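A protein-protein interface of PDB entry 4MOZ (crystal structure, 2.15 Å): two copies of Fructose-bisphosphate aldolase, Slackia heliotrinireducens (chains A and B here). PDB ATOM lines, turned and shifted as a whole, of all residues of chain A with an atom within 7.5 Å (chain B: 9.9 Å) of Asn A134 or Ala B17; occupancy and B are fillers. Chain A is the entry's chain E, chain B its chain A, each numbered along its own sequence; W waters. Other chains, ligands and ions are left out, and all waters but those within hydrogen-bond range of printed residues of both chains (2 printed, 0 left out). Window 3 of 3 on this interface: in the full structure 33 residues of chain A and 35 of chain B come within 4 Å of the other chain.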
ATOM      1  N   VAL A 128       5.191  23.767  12.555  1.00  0.00           N
ATOM      2  CA  VAL A 128       6.104  24.293  13.568  1.00  0.00           C
ATOM      3  C   VAL A 128       7.430  23.528  13.517  1.00  0.00           C
ATOM      4  O   VAL A 128       8.509  24.130  13.538  1.00  0.00           O
ATOM      5  CB  VAL A 128       5.491  24.202  14.983  1.00  0.00           C
ATOM      6  CG1 VAL A 128       6.413  24.836  16.014  1.00  0.00           C
ATOM      7  CG2 VAL A 128       4.124  24.870  15.021  1.00  0.00           C
ATOM      8  N   LEU A 129       7.333  22.204  13.430  1.00  0.00           N
ATOM      9  CA  LEU A 129       8.498  21.327  13.343  1.00  0.00           C
ATOM     10  C   LEU A 129       9.398  21.656  12.148  1.00  0.00           C
ATOM     11  O   LEU A 129      10.624  21.606  12.264  1.00  0.00           O
ATOM     12  CB  LEU A 129       8.046  19.862  13.275  1.00  0.00           C
ATOM     13  CG  LEU A 129       7.976  18.996  14.540  1.00  0.00           C
ATOM     14  CD1 LEU A 129       7.428  19.730  15.758  1.00  0.00           C
ATOM     15  CD2 LEU A 129       7.172  17.737  14.261  1.00  0.00           C
ATOM     16  N   ALA A 130       8.782  21.990  11.010  1.00  0.00           N
ATOM     17  CA  ALA A 130       9.518  22.334   9.787  1.00  0.00           C
ATOM     18  C   ALA A 130      10.256  23.659   9.945  1.00  0.00           C
ATOM     19  O   ALA A 130      11.355  23.837   9.414  1.00  0.00           O
ATOM     20  CB  ALA A 130       8.580  22.392   8.589  1.00  0.00           C
ATOM     21  N   MET A 131       9.640  24.582  10.680  1.00  0.00           N
ATOM     22  CA  MET A 131      10.251  25.870  10.962  1.00  0.00           C
ATOM     23  C   MET A 131      11.419  25.689  11.931  1.00  0.00           C
ATOM     24  O   MET A 131      12.477  26.297  11.754  1.00  0.00           O
ATOM     25  CB  MET A 131       9.210  26.829  11.525  1.00  0.00           C
ATOM     26  CG  MET A 131       9.452  28.277  11.175  1.00  0.00           C
ATOM     27  SD  MET A 131       7.963  29.422  11.722  1.00  0.00           S
ATOM     28  CE  MET A 131       8.096  29.210  13.662  1.00  0.00           C
ATOM     29  N   ARG A 132      11.223  24.841  12.943  1.00  0.00           N
ATOM     30  CA  ARG A 132      12.300  24.445  13.857  1.00  0.00           C
ATOM     31  C   ARG A 132      13.492  23.883  13.074  1.00  0.00           C
ATOM     32  O   ARG A 132      14.629  24.312  13.275  1.00  0.00           O
ATOM     33  CB  ARG A 132      11.796  23.415  14.879  1.00  0.00           C
ATOM     34  CG  ARG A 132      12.856  22.926  15.866  1.00  0.00           C
ATOM     35  CD  ARG A 132      12.515  21.553  16.436  1.00  0.00           C
ATOM     36  NE  ARG A 132      12.407  20.536  15.389  1.00  0.00           N
ATOM     37  CZ  ARG A 132      11.818  19.351  15.535  1.00  0.00           C
ATOM     38  NH1 ARG A 132      11.267  19.007  16.691  1.00  0.00           N
ATOM     39  NH2 ARG A 132      11.774  18.505  14.513  1.00  0.00           N
ATOM     40  N   ASP A 133      13.217  22.946  12.170  1.00  0.00           N
ATOM     41  CA  ASP A 133      14.254  22.305  11.350  1.00  0.00           C
ATOM     42  C   ASP A 133      14.870  23.248  10.314  1.00  0.00           C
ATOM     43  O   ASP A 133      15.864  22.907   9.671  1.00  0.00           O
ATOM     44  CB  ASP A 133      13.698  21.048  10.667  1.00  0.00           C
ATOM     45  CG  ASP A 133      13.295  19.969  11.662  1.00  0.00           C
ATOM     46  OD1 ASP A 133      13.840  19.946  12.785  1.00  0.00           O
ATOM     47  OD2 ASP A 133      12.431  19.136  11.320  1.00  0.00           O
ATOM     48  N   ASN A 134      14.270  24.429  10.163  1.00  0.00           N
ATOM     49  CA  ASN A 134      14.808  25.480   9.305  1.00  0.00           C
ATOM     50  C   ASN A 134      15.620  26.493  10.117  1.00  0.00           C
ATOM     51  O   ASN A 134      16.014  27.538   9.607  1.00  0.00           O
ATOM     52  CB  ASN A 134      13.673  26.179   8.543  1.00  0.00           C
ATOM     53  CG  ASN A 134      14.143  26.858   7.267  1.00  0.00           C
ATOM     54  OD1 ASN A 134      15.109  26.430   6.632  1.00  0.00           O
ATOM     55  ND2 ASN A 134      13.450  27.919   6.878  1.00  0.00           N
ATOM     56  N   GLY A 135      15.858  26.183  11.390  1.00  0.00           N
ATOM     57  CA  GLY A 135      16.746  26.991  12.223  1.00  0.00           C
ATOM     58  C   GLY A 135      16.092  27.953  13.202  1.00  0.00           C
ATOM     59  O   GLY A 135      16.783  28.747  13.845  1.00  0.00           O
ATOM     60  N   VAL A 136      14.769  27.902  13.329  1.00  0.00           N
ATOM     61  CA  VAL A 136      14.095  28.750  14.313  1.00  0.00           C
ATOM     62  C   VAL A 136      14.123  28.085  15.688  1.00  0.00           C
ATOM     63  O   VAL A 136      13.730  26.933  15.845  1.00  0.00           O
ATOM     64  CB  VAL A 136      12.656  29.115  13.893  1.00  0.00           C
ATOM     65  CG1 VAL A 136      11.988  29.986  14.953  1.00  0.00           C
ATOM     66  CG2 VAL A 136      12.671  29.836  12.557  1.00  0.00           C
ATOM     67  N   ASN A 137      14.602  28.827  16.678  1.00  0.00           N
ATOM     68  CA  ASN A 137      14.710  28.336  18.041  1.00  0.00           C
ATOM     69  C   ASN A 137      13.340  28.238  18.735  1.00  0.00           C
ATOM     70  O   ASN A 137      13.007  29.039  19.619  1.00  0.00           O
ATOM     71  CB  ASN A 137      15.683  29.220  18.829  1.00  0.00           C
ATOM     72  CG  ASN A 137      16.030  28.645  20.186  1.00  0.00           C
ATOM     73  OD1 ASN A 137      16.233  27.439  20.335  1.00  0.00           O
ATOM     74  ND2 ASN A 137      16.104  29.513  21.186  1.00  0.00           N
ATOM     75  N   VAL B  11      12.985  36.414   2.661  1.00  0.00           N
ATOM     76  CA  VAL B  11      12.427  35.077   2.728  1.00  0.00           C
ATOM     77  C   VAL B  11      12.064  34.775   4.183  1.00  0.00           C
ATOM     78  O   VAL B  11      12.937  34.793   5.048  1.00  0.00           O
ATOM     79  CB  VAL B  11      13.425  34.031   2.189  1.00  0.00           C
ATOM     80  CG1 VAL B  11      12.800  32.648   2.188  1.00  0.00           C
ATOM     81  CG2 VAL B  11      13.890  34.404   0.785  1.00  0.00           C
ATOM     82  N   PRO B  12      10.768  34.520   4.462  1.00  0.00           N
ATOM     83  CA  PRO B  12      10.365  34.206   5.838  1.00  0.00           C
ATOM     84  C   PRO B  12      10.822  32.805   6.231  1.00  0.00           C
ATOM     85  O   PRO B  12      11.058  31.963   5.360  1.00  0.00           O
ATOM     86  CB  PRO B  12       8.837  34.296   5.792  1.00  0.00           C
ATOM     87  CG  PRO B  12       8.483  34.008   4.370  1.00  0.00           C
ATOM     88  CD  PRO B  12       9.630  34.485   3.522  1.00  0.00           C
ATOM     89  N   ALA B  13      10.939  32.563   7.534  1.00  0.00           N
ATOM     90  CA  ALA B  13      11.533  31.331   8.054  1.00  0.00           C
ATOM     91  C   ALA B  13      10.708  30.058   7.811  1.00  0.00           C
ATOM     92  O   ALA B  13      11.201  28.941   8.031  1.00  0.00           O
ATOM     93  CB  ALA B  13      11.852  31.491   9.530  1.00  0.00           C
ATOM     94  N   ASP B  14       9.466  30.218   7.357  1.00  0.00           N
ATOM     95  CA  ASP B  14       8.625  29.062   7.020  1.00  0.00           C
ATOM     96  C   ASP B  14       8.752  28.633   5.553  1.00  0.00           C
ATOM     97  O   ASP B  14       8.142  27.649   5.127  1.00  0.00           O
ATOM     98  CB  ASP B  14       7.159  29.290   7.420  1.00  0.00           C
ATOM     99  CG  ASP B  14       6.515  30.470   6.701  1.00  0.00           C
ATOM    100  OD1 ASP B  14       7.240  31.336   6.168  1.00  0.00           O
ATOM    101  OD2 ASP B  14       5.267  30.535   6.681  1.00  0.00           O
ATOM    102  N   VAL B  15       9.543  29.378   4.783  1.00  0.00           N
ATOM    103  CA  VAL B  15       9.959  28.922   3.459  1.00  0.00           C
ATOM    104  C   VAL B  15      11.211  28.083   3.674  1.00  0.00           C
ATOM    105  O   VAL B  15      12.260  28.605   4.036  1.00  0.00           O
ATOM    106  CB  VAL B  15      10.234  30.092   2.485  1.00  0.00           C
ATOM    107  CG1 VAL B  15      10.790  29.585   1.161  1.00  0.00           C
ATOM    108  CG2 VAL B  15       8.973  30.906   2.251  1.00  0.00           C
ATOM    109  N   LEU B  16      11.080  26.776   3.474  1.00  0.00           N
ATOM    110  CA  LEU B  16      12.168  25.832   3.720  1.00  0.00           C
ATOM    111  C   LEU B  16      13.287  25.956   2.687  1.00  0.00           C
ATOM    112  O   LEU B  16      13.080  26.485   1.585  1.00  0.00           O
ATOM    113  CB  LEU B  16      11.629  24.396   3.774  1.00  0.00           C
ATOM    114  CG  LEU B  16      10.365  24.170   4.620  1.00  0.00           C
ATOM    115  CD1 LEU B  16       9.883  22.727   4.533  1.00  0.00           C
ATOM    116  CD2 LEU B  16      10.568  24.596   6.073  1.00  0.00           C
ATOM    117  N   ALA B  17      14.464  25.457   3.056  1.00  0.00           N
ATOM    118  CA  ALA B  17      15.680  25.606   2.254  1.00  0.00           C
ATOM    119  C   ALA B  17      15.511  25.166   0.806  1.00  0.00           C
ATOM    120  O   ALA B  17      15.962  25.860  -0.101  1.00  0.00           O
ATOM    121  CB  ALA B  17      16.851  24.875   2.907  1.00  0.00           C
ATOM    122  N   ASP B  18      14.852  24.033   0.584  1.00  0.00           N
ATOM    123  CA  ASP B  18      14.688  23.514  -0.774  1.00  0.00           C
ATOM    124  C   ASP B  18      13.617  24.250  -1.600  1.00  0.00           C
ATOM    125  O   ASP B  18      13.443  23.968  -2.785  1.00  0.00           O
ATOM    126  CB  ASP B  18      14.446  21.997  -0.758  1.00  0.00           C
ATOM    127  CG  ASP B  18      13.136  21.611  -0.085  1.00  0.00           C
ATOM    128  OD1 ASP B  18      12.654  22.366   0.792  1.00  0.00           O
ATOM    129  OD2 ASP B  18      12.590  20.540  -0.429  1.00  0.00           O
ATOM    130  N   ALA B  19      12.915  25.192  -0.972  1.00  0.00           N
ATOM    131  CA  ALA B  19      11.875  25.974  -1.646  1.00  0.00           C
ATOM    132  C   ALA B  19      12.228  27.465  -1.739  1.00  0.00           C
ATOM    133  O   ALA B  19      11.449  28.263  -2.265  1.00  0.00           O
ATOM    134  CB  ALA B  19      10.536  25.785  -0.942  1.00  0.00           C
ATOM    135  N   ARG B  20      13.405  27.825  -1.236  1.00  0.00           N
ATOM    136  CA  ARG B  20      13.854  29.222  -1.178  1.00  0.00           C
ATOM    137  C   ARG B  20      13.914  29.906  -2.550  1.00  0.00           C
ATOM    138  O   ARG B  20      13.394  31.012  -2.721  1.00  0.00           O
ATOM    139  CB  ARG B  20      15.219  29.313  -0.487  1.00  0.00           C
ATOM    140  CG  ARG B  20      15.683  30.736  -0.233  1.00  0.00           C
ATOM    141  CD  ARG B  20      16.991  30.789   0.538  1.00  0.00           C
ATOM    142  NE  ARG B  20      17.297  32.160   0.948  1.00  0.00           N
ATOM    143  CZ  ARG B  20      16.894  32.719   2.090  1.00  0.00           C
ATOM    144  NH1 ARG B  20      16.167  32.029   2.963  1.00  0.00           N
ATOM    145  NH2 ARG B  20      17.222  33.975   2.360  1.00  0.00           N
ATOM    146  N   GLU B  21      14.550  29.249  -3.516  1.00  0.00           N
ATOM    147  CA  GLU B  21      14.726  29.837  -4.840  1.00  0.00           C
ATOM    148  C   GLU B  21      13.396  29.969  -5.573  1.00  0.00           C
ATOM    149  O   GLU B  21      13.161  30.962  -6.263  1.00  0.00           O
ATOM    150  CB  GLU B  21      15.746  29.050  -5.671  1.00  0.00           C
ATOM    151  CG  GLU B  21      17.156  29.024  -5.086  1.00  0.00           C
ATOM    152  CD  GLU B  21      17.686  30.403  -4.693  1.00  0.00           C
ATOM    153  OE1 GLU B  21      17.556  31.366  -5.484  1.00  0.00           O
ATOM    154  OE2 GLU B  21      18.247  30.525  -3.582  1.00  0.00           O
ATOM    155  N   THR B  22      12.530  28.971  -5.399  1.00  0.00           N
ATOM    156  CA  THR B  22      11.178  29.005  -5.949  1.00  0.00           C
ATOM    157  C   THR B  22      10.386  30.181  -5.373  1.00  0.00           C
ATOM    158  O   THR B  22       9.754  30.928  -6.123  1.00  0.00           O
ATOM    159  CB  THR B  22      10.433  27.670  -5.724  1.00  0.00           C
ATOM    160  OG1 THR B  22      11.136  26.617  -6.390  1.00  0.00           O
ATOM    161  CG2 THR B  22       9.007  27.730  -6.277  1.00  0.00           C
ATOM    162  N   TYR B  23      10.436  30.353  -4.052  1.00  0.00           N
ATOM    163  CA  TYR B  23       9.734  31.466  -3.402  1.00  0.00           C
ATOM    164  C   TYR B  23      10.178  32.813  -3.973  1.00  0.00           C
ATOM    165  O   TYR B  23       9.342  33.670  -4.261  1.00  0.00           O
ATOM    166  CB  TYR B  23       9.921  31.439  -1.879  1.00  0.00           C
ATOM    167  CG  TYR B  23       9.317  32.629  -1.165  1.00  0.00           C
ATOM    168  CD1 TYR B  23       7.969  32.636  -0.789  1.00  0.00           C
ATOM    169  CD2 TYR B  23      10.092  33.751  -0.857  1.00  0.00           C
ATOM    170  CE1 TYR B  23       7.411  33.726  -0.132  1.00  0.00           C
ATOM    171  CE2 TYR B  23       9.543  34.846  -0.199  1.00  0.00           C
ATOM    172  CZ  TYR B  23       8.206  34.829   0.162  1.00  0.00           C
ATOM    173  OH  TYR B  23       7.663  35.916   0.810  1.00  0.00           O
ATOM    174  N   ILE B  24      11.491  32.982  -4.127  1.00  0.00           N
ATOM    175  CA  ILE B  24      12.057  34.218  -4.668  1.00  0.00           C
ATOM    176  C   ILE B  24      11.609  34.409  -6.115  1.00  0.00           C
ATOM    177  O   ILE B  24      11.188  35.502  -6.486  1.00  0.00           O
ATOM    178  CB  ILE B  24      13.598  34.273  -4.523  1.00  0.00           C
ATOM    179  CG1 ILE B  24      13.990  34.282  -3.038  1.00  0.00           C
ATOM    180  CG2 ILE B  24      14.169  35.509  -5.208  1.00  0.00           C
ATOM    181  CD1 ILE B  24      15.435  33.909  -2.760  1.00  0.00           C
ATOM    182  N   HIS B 167       4.080  28.013   1.773  1.00  0.00           N
ATOM    183  CA  HIS B 167       5.470  28.405   1.943  1.00  0.00           C
ATOM    184  C   HIS B 167       6.403  27.235   1.913  1.00  0.00           C
ATOM    185  O   HIS B 167       7.547  27.367   1.483  1.00  0.00           O
ATOM    186  CB  HIS B 167       5.655  29.242   3.204  1.00  0.00           C
ATOM    187  CG  HIS B 167       5.145  30.660   3.063  1.00  0.00           C
ATOM    188  ND1 HIS B 167       4.772  31.408   4.118  1.00  0.00           N
ATOM    189  CD2 HIS B 167       4.933  31.443   1.932  1.00  0.00           C
ATOM    190  CE1 HIS B 167       4.353  32.612   3.686  1.00  0.00           C
ATOM    191  NE2 HIS B 167       4.452  32.631   2.349  1.00  0.00           N
ATOM    192  N   GLU B 168       5.912  26.076   2.349  1.00  0.00           N
ATOM    193  CA  GLU B 168       6.637  24.817   2.203  1.00  0.00           C
ATOM    194  C   GLU B 168       6.959  24.559   0.730  1.00  0.00           C
ATOM    195  O   GLU B 168       8.009  24.006   0.399  1.00  0.00           O
ATOM    196  CB  GLU B 168       5.805  23.665   2.771  1.00  0.00           C
ATOM    197  CG  GLU B 168       6.476  22.300   2.717  1.00  0.00           C
ATOM    198  CD  GLU B 168       5.587  21.169   3.209  1.00  0.00           C
ATOM    199  OE1 GLU B 168       4.460  21.429   3.686  1.00  0.00           O
ATOM    200  OE2 GLU B 168       6.021  20.004   3.113  1.00  0.00           O
ATOM    201  N   GLU B 169       6.045  24.966  -0.146  1.00  0.00           N
ATOM    202  CA  GLU B 169       6.200  24.767  -1.586  1.00  0.00           C
ATOM    203  C   GLU B 169       6.771  26.001  -2.286  1.00  0.00           C
ATOM    204  O   GLU B 169       6.935  26.006  -3.505  1.00  0.00           O
ATOM    205  CB  GLU B 169       4.861  24.359  -2.215  1.00  0.00           C
ATOM    206  CG  GLU B 169       4.312  23.026  -1.722  1.00  0.00           C
ATOM    207  CD  GLU B 169       5.115  21.816  -2.191  1.00  0.00           C
ATOM    208  OE1 GLU B 169       5.830  21.901  -3.218  1.00  0.00           O
ATOM    209  OE2 GLU B 169       5.017  20.762  -1.530  1.00  0.00           O
ATOM    210  N   GLY B 170       7.073  27.040  -1.513  1.00  0.00           N
ATOM    211  CA  GLY B 170       7.612  28.283  -2.061  1.00  0.00           C
ATOM    212  C   GLY B 170       6.620  29.072  -2.901  1.00  0.00           C
ATOM    213  O   GLY B 170       7.002  29.743  -3.865  1.00  0.00           O
HETATM  214  O   HOH W   1      14.027  30.505   4.826  1.00  0.00           O
HETATM  215  O   HOH W   2      14.467  23.697   5.483  1.00  0.00           O
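ND2 of Asn A134 is in hydrogen-bond range of O of Ala B13, at 2.7 Å. The side-chain amide nitrogen (ND2) of Asn A134 sits at hydrogen-bond distance from the backbone carbonyl oxygen (O) of Val B15 (3.2 Å).
N of Val A136 sits at hydrogen-bond distance from O of Met A131 (3.2 Å).
Among the printed residues, pairs that only touch across the chains: Ala A130 with Leu B16 (3.5 Å), Val A136 with Ala B13 (3.5 Å), Met A131 with Ala B13 (3.7 Å), Asn A134 with Ala B17 (3.8 Å) and Asn A134 with Leu B16 (3.997 Å).
Printed residues of chain B within 4 Å of Asn A134: Ala B13, Val B15, Leu B16 and Ala B17. Ala B17 touches just one residue of chain A: Asn A134 (3.8 Å). No residue of chain B comes within 4 Å of Asp A133. Gly A135 touches none of the printed residues of chain B. Of the printed residues of chain A, Leu B16 touches Ala A130 and Asn A134. Of the printed residues of chain B, Met A131 touches Ala B13. Of the printed residues of chain B, Val A136 touches Ala B13. Printed residues of chain A within 4 Å of Val B15: Asn A134 (3.2 Å). The nearest printed residue of chain A that does not touch Ala B13 is Ala A130 (5.3 Å).
Printed residues of chain B that touch a printed residue of chain A: Ala B13, Val B15, Leu B16 and Ala B17. Hydrophobic or aromatic side chains of chain B within 4 Å of the printed part of chain A: Ala B13 and Leu B16. Printed residues of chain A that touch a printed residue of chain B: Ala A130, Met A131, Asn A134 and Val A136. Hydrophobic or aromatic side chains of chain A within 4 Å of the printed part of chain B: Ala A130, Met A131 and Val A136. Among the printed residues, 7 pairs touch across the chains. Among the printed residues, no Asp or Glu carboxylate lies within 4 Å of a Lys or Arg side-chain nitrogen of the other chain.
No position is printed for both chains. Of the 7 pairs that touch across the chains among the printed residues, none has its exchanged pair printed and touching as well.
Water W1 lies within hydrogen-bond range of the backbone carbonyl oxygen of Val B15 (2.7 Å), the guanidinium group of Arg B20 (3.2 Å), the backbone carbonyl oxygen of Pro B12 (3.4 Å) and the side-chain amide nitrogen of Asn A134 (3.4 Å). Water W2 lies within hydrogen-bond range of N of Ala B17 and OD1 of Asn A134.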
